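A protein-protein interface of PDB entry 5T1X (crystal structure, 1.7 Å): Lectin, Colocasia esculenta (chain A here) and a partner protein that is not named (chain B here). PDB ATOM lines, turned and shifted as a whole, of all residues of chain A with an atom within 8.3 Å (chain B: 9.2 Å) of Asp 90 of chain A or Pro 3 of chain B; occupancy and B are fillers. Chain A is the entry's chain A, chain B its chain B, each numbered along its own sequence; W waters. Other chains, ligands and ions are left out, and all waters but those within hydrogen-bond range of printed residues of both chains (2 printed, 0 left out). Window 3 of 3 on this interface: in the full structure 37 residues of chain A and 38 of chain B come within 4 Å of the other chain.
Thr 108 of chain B touches Leu 35 of chain A.
CG2 of Ile 2 of chain B touches CE1 of His 88 of chain A (3.8 Å).
Phe 10 of chain B touches His 88 of chain A.
Pro 89 of chain A touches Pro 3 of chain B (CG to O, 3.5 Å).
Thr 5 of chain B touches Pro 89 of chain A.
Phe 10 of chain B touches Pro 89 of chain A.
Asp 90 of chain A touches Pro 3 of chain B (OD1 to CD, 3.6 Å).
Thr 108 of chain B touches Arg 92 of chain A.
O of Ser 109 of chain B touches CD of Arg 92 of chain A, 3.6 Å away.
Water W1 lies within hydrogen-bond range of the side-chain amide oxygen (OD1) of Asn 20 of chain A, the backbone carbonyl oxygen (O) of Phe 4 of chain B and the side-chain hydroxyl (OG1) of Thr 5 of chain B.
Water W2 lies within hydrogen-bond range of the side-chain hydroxyl (OG1) of Thr 108 of chain B (2.7 Å), the backbone carbonyl oxygen (O) of Gly 38 of chain A (2.7 Å) and the backbone carbonyl oxygen (O) of Gly 91 of chain A (2.8 Å).
Of the 13 printed residues of chain B, 6 touch a printed residue of chain A.
Printed residues of chain B that touch a printed residue of chain A: Ile 2, Pro 3, Thr 5, Phe 10, Thr 108 and Ser 109.
Hydrophobic or aromatic side chains of chain B within 4 Å of the printed part of chain A: Ile 2, Pro 3 and Phe 10.
Along chain B the printed residues that touch a printed residue of chain A span positions 2 to 109.
Of the 13 printed residues of chain A, 7 touch a printed residue of chain B.
Printed residues of chain A that touch a printed residue of chain B: Asn 20, Leu 35, His 88, Pro 89, Asp 90, Arg 92 and Leu 93.
Hydrophobic or aromatic side chains of chain A within 4 Å of the printed part of chain B: Leu 35, His 88, Pro 89 and Leu 93.
Along chain A the printed residues that touch a printed residue of chain B span positions 20 to 93.
Printed residues of chain B within 4 Å of Asn 20 of chain A: Thr 5 (3.1 Å).
Of the printed residues of chain B, His 88 of chain A touches Ile 2 (3.8 Å) and Phe 10 (3.6 Å).
Pro 89 of chain A touches just these residues of chain B: Pro 3 (3.5 Å), Thr 5 (3.9 Å) and Phe 10 (3.7 Å).
Asp 90 of chain A touches one residue of chain B.
Pro 3 of chain B touches two residues of chain A.
Printed residues of chain A within 4 Å of Thr 5 of chain B: Asn 20 (3.1 Å) and Pro 89 (3.9 Å).
Of the printed residues of chain A, Phe 10 of chain B touches His 88 (3.6 Å) and Pro 89 (3.7 Å).
Printed residues of chain A within 4 Å of Ser 109 of chain B: Arg 92 (3.6 Å).
The nearest residue of chain B that does not touch Asp 90 of chain A is Ile 2 of chain B (4.5 Å).
The side-chain hydroxyl of Thr 5 of chain B lies within hydrogen-bond range of the side-chain amide nitrogen of Asn 20 of chain A, 3.1 Å away.
The side-chain hydroxyl of Thr 108 of chain B sits at hydrogen-bond distance from the backbone NH of Leu 93 of chain A.
The side-chain amide oxygen of Gln 13 of chain B lies within hydrogen-bond range of the backbone NH of Phe 10 of chain B.
O of Ile 2 of chain B lies within hydrogen-bond range of NE2 of Gln 13 of chain B.
The backbone carbonyl oxygen (O) of Pro 3 of chain B is in hydrogen-bond range of the side-chain amide nitrogen (NE2) of Gln 13 of chain B.
The side-chain amide nitrogen of Asn 20 of chain A sits at hydrogen-bond distance from the backbone carbonyl oxygen of Leu 87 of chain A, 2.9 Å away.
The backbone NH of Asp 90 of chain A lies within hydrogen-bond range of a ring nitrogen (ND1) of His 88 of chain A, 2.9 Å away.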
ATOM      1  N   ASN A  20     -26.390   3.935 -12.036  1.00  0.00           N
ATOM      2  CA  ASN A  20     -26.442   5.382 -12.228  1.00  0.00           C
ATOM      3  C   ASN A  20     -27.835   5.693 -12.795  1.00  0.00           C
ATOM      4  O   ASN A  20     -28.108   5.400 -13.958  1.00  0.00           O
ATOM      5  CB  ASN A  20     -25.287   5.905 -13.095  1.00  0.00           C
ATOM      6  CG  ASN A  20     -25.110   7.403 -12.977  1.00  0.00           C
ATOM      7  OD1 ASN A  20     -26.018   8.138 -12.578  1.00  0.00           O
ATOM      8  ND2 ASN A  20     -23.955   7.899 -13.372  1.00  0.00           N
ATOM      9  N   GLY A  21     -28.726   6.193 -11.928  1.00  0.00           N
ATOM     10  CA  GLY A  21     -30.115   6.456 -12.288  1.00  0.00           C
ATOM     11  C   GLY A  21     -30.819   5.152 -12.621  1.00  0.00           C
ATOM     12  O   GLY A  21     -30.701   4.183 -11.873  1.00  0.00           O
ATOM     13  N   PHE A  23     -30.036   3.121 -15.038  1.00  0.00           N
ATOM     14  CA  PHE A  23     -29.068   2.201 -15.630  1.00  0.00           C
ATOM     15  C   PHE A  23     -28.416   1.368 -14.550  1.00  0.00           C
ATOM     16  O   PHE A  23     -27.846   1.909 -13.597  1.00  0.00           O
ATOM     17  CB  PHE A  23     -28.061   2.982 -16.477  1.00  0.00           C
ATOM     18  CG  PHE A  23     -28.786   3.811 -17.514  1.00  0.00           C
ATOM     19  CD1 PHE A  23     -29.386   3.208 -18.618  1.00  0.00           C
ATOM     20  CD2 PHE A  23     -28.921   5.186 -17.358  1.00  0.00           C
ATOM     21  CE1 PHE A  23     -30.081   3.974 -19.562  1.00  0.00           C
ATOM     22  CE2 PHE A  23     -29.614   5.950 -18.305  1.00  0.00           C
ATOM     23  CZ  PHE A  23     -30.179   5.340 -19.405  1.00  0.00           C
ATOM     24  N   LEU A  35     -26.311  -4.777 -18.737  1.00  0.00           N
ATOM     25  CA  LEU A  35     -26.527  -3.369 -18.446  1.00  0.00           C
ATOM     26  C   LEU A  35     -28.003  -3.078 -18.683  1.00  0.00           C
ATOM     27  O   LEU A  35     -28.412  -2.800 -19.814  1.00  0.00           O
ATOM     28  CB  LEU A  35     -25.599  -2.471 -19.289  1.00  0.00           C
ATOM     29  CG  LEU A  35     -25.631  -0.966 -18.972  1.00  0.00           C
ATOM     30  CD1 LEU A  35     -25.396  -0.697 -17.497  1.00  0.00           C
ATOM     31  CD2 LEU A  35     -24.591  -0.221 -19.786  1.00  0.00           C
ATOM     32  N   ASN A  37     -31.410  -1.425 -19.151  1.00  0.00           N
ATOM     33  CA  ASN A  37     -31.881  -0.187 -19.787  1.00  0.00           C
ATOM     34  C   ASN A  37     -30.798   0.446 -20.682  1.00  0.00           C
ATOM     35  O   ASN A  37     -31.047   1.490 -21.287  1.00  0.00           O
ATOM     36  CB  ASN A  37     -32.425   0.835 -18.766  1.00  0.00           C
ATOM     37  CG  ASN A  37     -33.638   0.331 -18.029  1.00  0.00           C
ATOM     38  OD1 ASN A  37     -34.621  -0.113 -18.630  1.00  0.00           O
ATOM     39  ND2 ASN A  37     -33.588   0.367 -16.706  1.00  0.00           N
ATOM     40  N   GLY A  38     -29.643  -0.214 -20.790  1.00  0.00           N
ATOM     41  CA  GLY A  38     -28.526   0.241 -21.611  1.00  0.00           C
ATOM     42  C   GLY A  38     -28.306  -0.562 -22.881  1.00  0.00           C
ATOM     43  O   GLY A  38     -27.322  -0.329 -23.590  1.00  0.00           O
ATOM     44  N   LEU A  87     -20.024   3.900 -14.938  1.00  0.00           N
ATOM     45  CA  LEU A  87     -21.362   3.837 -15.502  1.00  0.00           C
ATOM     46  C   LEU A  87     -21.823   5.292 -15.717  1.00  0.00           C
ATOM     47  O   LEU A  87     -22.186   6.002 -14.770  1.00  0.00           O
ATOM     48  CB  LEU A  87     -22.319   3.019 -14.623  1.00  0.00           C
ATOM     49  CG  LEU A  87     -23.757   2.836 -15.131  1.00  0.00           C
ATOM     50  CD1 LEU A  87     -23.810   2.422 -16.593  1.00  0.00           C
ATOM     51  CD2 LEU A  87     -24.500   1.823 -14.288  1.00  0.00           C
ATOM     52  N   HIS A  88     -21.762   5.728 -16.987  1.00  0.00           N
ATOM     53  CA  HIS A  88     -22.158   7.067 -17.428  1.00  0.00           C
ATOM     54  C   HIS A  88     -23.671   7.254 -17.232  1.00  0.00           C
ATOM     55  O   HIS A  88     -24.423   6.302 -17.480  1.00  0.00           O
ATOM     56  CB  HIS A  88     -21.774   7.248 -18.908  1.00  0.00           C
ATOM     57  CG  HIS A  88     -21.834   8.662 -19.399  1.00  0.00           C
ATOM     58  ND1 HIS A  88     -23.039   9.263 -19.720  1.00  0.00           N
ATOM     59  CD2 HIS A  88     -20.825   9.522 -19.679  1.00  0.00           C
ATOM     60  CE1 HIS A  88     -22.731  10.481 -20.139  1.00  0.00           C
ATOM     61  NE2 HIS A  88     -21.412  10.680 -20.143  1.00  0.00           N
ATOM     62  N   PRO A  89     -24.150   8.462 -16.814  1.00  0.00           N
ATOM     63  CA  PRO A  89     -25.600   8.661 -16.612  1.00  0.00           C
ATOM     64  C   PRO A  89     -26.444   8.533 -17.890  1.00  0.00           C
ATOM     65  O   PRO A  89     -27.656   8.378 -17.782  1.00  0.00           O
ATOM     66  CB  PRO A  89     -25.682  10.094 -16.072  1.00  0.00           C
ATOM     67  CG  PRO A  89     -24.450  10.763 -16.600  1.00  0.00           C
ATOM     68  CD  PRO A  89     -23.406   9.689 -16.460  1.00  0.00           C
ATOM     69  N   ASP A  90     -25.825   8.619 -19.085  1.00  0.00           N
ATOM     70  CA  ASP A  90     -26.581   8.494 -20.345  1.00  0.00           C
ATOM     71  C   ASP A  90     -26.723   7.005 -20.776  1.00  0.00           C
ATOM     72  O   ASP A  90     -27.230   6.712 -21.862  1.00  0.00           O
ATOM     73  CB  ASP A  90     -25.997   9.392 -21.463  1.00  0.00           C
ATOM     74  CG  ASP A  90     -26.330  10.876 -21.290  1.00  0.00           C
ATOM     75  OD1 ASP A  90     -27.469  11.192 -20.859  1.00  0.00           O
ATOM     76  OD2 ASP A  90     -25.452  11.723 -21.575  1.00  0.00           O
ATOM     77  N   GLY A  91     -26.333   6.086 -19.890  1.00  0.00           N
ATOM     78  CA  GLY A  91     -26.552   4.656 -20.078  1.00  0.00           C
ATOM     79  C   GLY A  91     -25.535   3.827 -20.823  1.00  0.00           C
ATOM     80  O   GLY A  91     -25.917   2.944 -21.602  1.00  0.00           O
ATOM     81  N   ARG A  92     -24.256   4.072 -20.566  1.00  0.00           N
ATOM     82  CA  ARG A  92     -23.167   3.290 -21.148  1.00  0.00           C
ATOM     83  C   ARG A  92     -22.088   3.051 -20.118  1.00  0.00           C
ATOM     84  O   ARG A  92     -21.840   3.919 -19.279  1.00  0.00           O
ATOM     85  CB  ARG A  92     -22.578   3.927 -22.430  1.00  0.00           C
ATOM     86  CG  ARG A  92     -22.078   5.354 -22.316  1.00  0.00           C
ATOM     87  CD  ARG A  92     -21.750   5.919 -23.691  1.00  0.00           C
ATOM     88  NE  ARG A  92     -21.054   7.204 -23.592  1.00  0.00           N
ATOM     89  CZ  ARG A  92     -21.657   8.387 -23.515  1.00  0.00           C
ATOM     90  NH1 ARG A  92     -22.982   8.469 -23.525  1.00  0.00           N
ATOM     91  NH2 ARG A  92     -20.938   9.497 -23.422  1.00  0.00           N
ATOM     92  N   LEU A  93     -21.456   1.867 -20.168  1.00  0.00           N
ATOM     93  CA  LEU A  93     -20.325   1.549 -19.298  1.00  0.00           C
ATOM     94  C   LEU A  93     -19.083   1.881 -20.099  1.00  0.00           C
ATOM     95  O   LEU A  93     -18.953   1.437 -21.241  1.00  0.00           O
ATOM     96  CB  LEU A  93     -20.343   0.082 -18.821  1.00  0.00           C
ATOM     97  CG  LEU A  93     -19.136  -0.375 -17.995  1.00  0.00           C
ATOM     98  CD1 LEU A  93     -19.152   0.237 -16.595  1.00  0.00           C
ATOM     99  CD2 LEU A  93     -19.083  -1.887 -17.915  1.00  0.00           C
ATOM    100  N   ASN B   1     -26.382  19.265 -22.294  1.00  0.00           N
ATOM    101  CA  ASN B   1     -25.578  19.082 -21.091  1.00  0.00           C
ATOM    102  C   ASN B   1     -25.685  17.659 -20.577  1.00  0.00           C
ATOM    103  O   ASN B   1     -26.733  17.038 -20.700  1.00  0.00           O
ATOM    104  CB  ASN B   1     -26.005  20.052 -19.993  1.00  0.00           C
ATOM    105  CG  ASN B   1     -25.818  21.504 -20.354  1.00  0.00           C
ATOM    106  OD1 ASN B   1     -25.964  21.910 -21.509  1.00  0.00           O
ATOM    107  ND2 ASN B   1     -25.558  22.320 -19.352  1.00  0.00           N
ATOM    108  N   ILE B   2     -24.608  17.166 -19.963  1.00  0.00           N
ATOM    109  CA  ILE B   2     -24.561  15.817 -19.393  1.00  0.00           C
ATOM    110  C   ILE B   2     -25.234  15.846 -18.012  1.00  0.00           C
ATOM    111  O   ILE B   2     -24.885  16.723 -17.208  1.00  0.00           O
ATOM    112  CB  ILE B   2     -23.072  15.357 -19.299  1.00  0.00           C
ATOM    113  CG1 ILE B   2     -22.391  15.355 -20.690  1.00  0.00           C
ATOM    114  CG2 ILE B   2     -22.920  13.987 -18.590  1.00  0.00           C
ATOM    115  CD1 ILE B   2     -20.830  15.555 -20.656  1.00  0.00           C
ATOM    116  N   PRO B   3     -26.129  14.883 -17.668  1.00  0.00           N
ATOM    117  CA  PRO B   3     -26.701  14.872 -16.312  1.00  0.00           C
ATOM    118  C   PRO B   3     -25.608  14.756 -15.255  1.00  0.00           C
ATOM    119  O   PRO B   3     -24.574  14.123 -15.483  1.00  0.00           O
ATOM    120  CB  PRO B   3     -27.611  13.639 -16.316  1.00  0.00           C
ATOM    121  CG  PRO B   3     -27.934  13.415 -17.750  1.00  0.00           C
ATOM    122  CD  PRO B   3     -26.659  13.761 -18.470  1.00  0.00           C
ATOM    123  N   PHE B   4     -25.815  15.416 -14.123  1.00  0.00           N
ATOM    124  CA  PHE B   4     -24.824  15.389 -13.069  1.00  0.00           C
ATOM    125  C   PHE B   4     -24.887  14.100 -12.243  1.00  0.00           C
ATOM    126  O   PHE B   4     -25.971  13.598 -11.942  1.00  0.00           O
ATOM    127  CB  PHE B   4     -25.007  16.611 -12.153  1.00  0.00           C
ATOM    128  CG  PHE B   4     -23.935  16.758 -11.107  1.00  0.00           C
ATOM    129  CD1 PHE B   4     -22.616  17.024 -11.470  1.00  0.00           C
ATOM    130  CD2 PHE B   4     -24.240  16.642  -9.756  1.00  0.00           C
ATOM    131  CE1 PHE B   4     -21.621  17.149 -10.499  1.00  0.00           C
ATOM    132  CE2 PHE B   4     -23.245  16.777  -8.786  1.00  0.00           C
ATOM    133  CZ  PHE B   4     -21.943  17.029  -9.165  1.00  0.00           C
ATOM    134  N   THR B   5     -23.707  13.597 -11.849  1.00  0.00           N
ATOM    135  CA  THR B   5     -23.559  12.469 -10.910  1.00  0.00           C
ATOM    136  C   THR B   5     -22.688  13.005  -9.770  1.00  0.00           C
ATOM    137  O   THR B   5     -21.680  13.659 -10.038  1.00  0.00           O
ATOM    138  CB  THR B   5     -22.999  11.229 -11.597  1.00  0.00           C
ATOM    139  OG1 THR B   5     -23.768  10.946 -12.770  1.00  0.00           O
ATOM    140  CG2 THR B   5     -22.990  10.011 -10.674  1.00  0.00           C
ATOM    141  N   ASP B   6     -23.088  12.775  -8.524  1.00  0.00           N
ATOM    142  CA  ASP B   6     -22.458  13.394  -7.353  1.00  0.00           C
ATOM    143  C   ASP B   6     -20.947  13.213  -7.233  1.00  0.00           C
ATOM    144  O   ASP B   6     -20.296  14.169  -6.830  1.00  0.00           O
ATOM    145  CB  ASP B   6     -23.118  12.942  -6.051  1.00  0.00           C
ATOM    146  CG  ASP B   6     -24.418  13.665  -5.722  1.00  0.00           C
ATOM    147  OD1 ASP B   6     -24.552  14.855  -6.094  1.00  0.00           O
ATOM    148  OD2 ASP B   6     -25.277  13.061  -5.042  1.00  0.00           O
ATOM    149  N   ASN B   7     -20.383  12.061  -7.601  1.00  0.00           N
ATOM    150  CA  ASN B   7     -18.940  11.820  -7.450  1.00  0.00           C
ATOM    151  C   ASN B   7     -18.139  11.916  -8.763  1.00  0.00           C
ATOM    152  O   ASN B   7     -16.955  11.578  -8.758  1.00  0.00           O
ATOM    153  CB  ASN B   7     -18.717  10.432  -6.825  1.00  0.00           C
ATOM    154  CG  ASN B   7     -19.249   9.291  -7.673  1.00  0.00           C
ATOM    155  OD1 ASN B   7     -20.178   9.454  -8.485  1.00  0.00           O
ATOM    156  ND2 ASN B   7     -18.683   8.102  -7.505  1.00  0.00           N
ATOM    157  N   LEU B   8     -18.771  12.359  -9.875  1.00  0.00           N
ATOM    158  CA  LEU B   8     -18.087  12.422 -11.171  1.00  0.00           C
ATOM    159  C   LEU B   8     -18.162  13.781 -11.823  1.00  0.00           C
ATOM    160  O   LEU B   8     -19.152  14.493 -11.659  1.00  0.00           O
ATOM    161  CB  LEU B   8     -18.732  11.422 -12.161  1.00  0.00           C
ATOM    162  CG  LEU B   8     -19.021   9.992 -11.697  1.00  0.00           C
ATOM    163  CD1 LEU B   8     -19.838   9.260 -12.743  1.00  0.00           C
ATOM    164  CD2 LEU B   8     -17.735   9.222 -11.400  1.00  0.00           C
ATOM    165  N   LEU B   9     -17.161  14.088 -12.652  1.00  0.00           N
ATOM    166  CA  LEU B   9     -17.135  15.269 -13.499  1.00  0.00           C
ATOM    167  C   LEU B   9     -16.559  14.851 -14.845  1.00  0.00           C
ATOM    168  O   LEU B   9     -15.370  14.564 -14.938  1.00  0.00           O
ATOM    169  CB  LEU B   9     -16.354  16.447 -12.868  1.00  0.00           C
ATOM    170  CG  LEU B   9     -16.627  17.812 -13.521  1.00  0.00           C
ATOM    171  CD1 LEU B   9     -17.982  18.343 -13.120  1.00  0.00           C
ATOM    172  CD2 LEU B   9     -15.557  18.817 -13.161  1.00  0.00           C
ATOM    173  N   PHE B  10     -17.422  14.725 -15.863  1.00  0.00           N
ATOM    174  CA  PHE B  10     -16.979  14.329 -17.193  1.00  0.00           C
ATOM    175  C   PHE B  10     -16.486  15.548 -17.953  1.00  0.00           C
ATOM    176  O   PHE B  10     -16.875  16.682 -17.622  1.00  0.00           O
ATOM    177  CB  PHE B  10     -18.124  13.651 -17.971  1.00  0.00           C
ATOM    178  CG  PHE B  10     -18.542  12.324 -17.402  1.00  0.00           C
ATOM    179  CD1 PHE B  10     -17.842  11.164 -17.713  1.00  0.00           C
ATOM    180  CD2 PHE B  10     -19.637  12.230 -16.543  1.00  0.00           C
ATOM    181  CE1 PHE B  10     -18.228   9.928 -17.177  1.00  0.00           C
ATOM    182  CE2 PHE B  10     -20.019  10.995 -16.006  1.00  0.00           C
ATOM    183  CZ  PHE B  10     -19.309   9.853 -16.324  1.00  0.00           C
ATOM    184  N   GLN B  13     -18.308  19.168 -18.427  1.00  0.00           N
ATOM    185  CA  GLN B  13     -19.158  19.637 -17.328  1.00  0.00           C
ATOM    186  C   GLN B  13     -18.463  20.791 -16.592  1.00  0.00           C
ATOM    187  O   GLN B  13     -17.234  20.886 -16.602  1.00  0.00           O
ATOM    188  CB  GLN B  13     -19.506  18.503 -16.353  1.00  0.00           C
ATOM    189  CG  GLN B  13     -20.347  17.410 -17.003  1.00  0.00           C
ATOM    190  CD  GLN B  13     -20.854  16.421 -15.990  1.00  0.00           C
ATOM    191  OE1 GLN B  13     -20.096  15.632 -15.416  1.00  0.00           O
ATOM    192  NE2 GLN B  13     -22.163  16.409 -15.794  1.00  0.00           N
ATOM    193  N   THR B 108     -19.768   0.435 -23.998  1.00  0.00           N
ATOM    194  CA  THR B 108     -20.840  -0.511 -24.345  1.00  0.00           C
ATOM    195  C   THR B 108     -21.617  -0.024 -25.569  1.00  0.00           C
ATOM    196  O   THR B 108     -22.079  -0.855 -26.354  1.00  0.00           O
ATOM    197  CB  THR B 108     -21.806  -0.749 -23.170  1.00  0.00           C
ATOM    198  OG1 THR B 108     -22.272   0.498 -22.661  1.00  0.00           O
ATOM    199  CG2 THR B 108     -21.192  -1.572 -22.063  1.00  0.00           C
ATOM    200  N   SER B 109     -21.758   1.308 -25.734  1.00  0.00           N
ATOM    201  CA  SER B 109     -22.521   1.905 -26.834  1.00  0.00           C
ATOM    202  C   SER B 109     -21.853   3.161 -27.401  1.00  0.00           C
ATOM    203  O   SER B 109     -21.304   3.972 -26.651  1.00  0.00           O
ATOM    204  CB  SER B 109     -23.935   2.248 -26.368  1.00  0.00           C
ATOM    205  OG  SER B 109     -24.714   2.816 -27.410  1.00  0.00           O
HETATM  206  O   HOH W   1     -26.763  10.742 -12.224  1.00  0.00           O
HETATM  207  O   HOH W   2     -24.896   0.929 -23.296  1.00  0.00           O
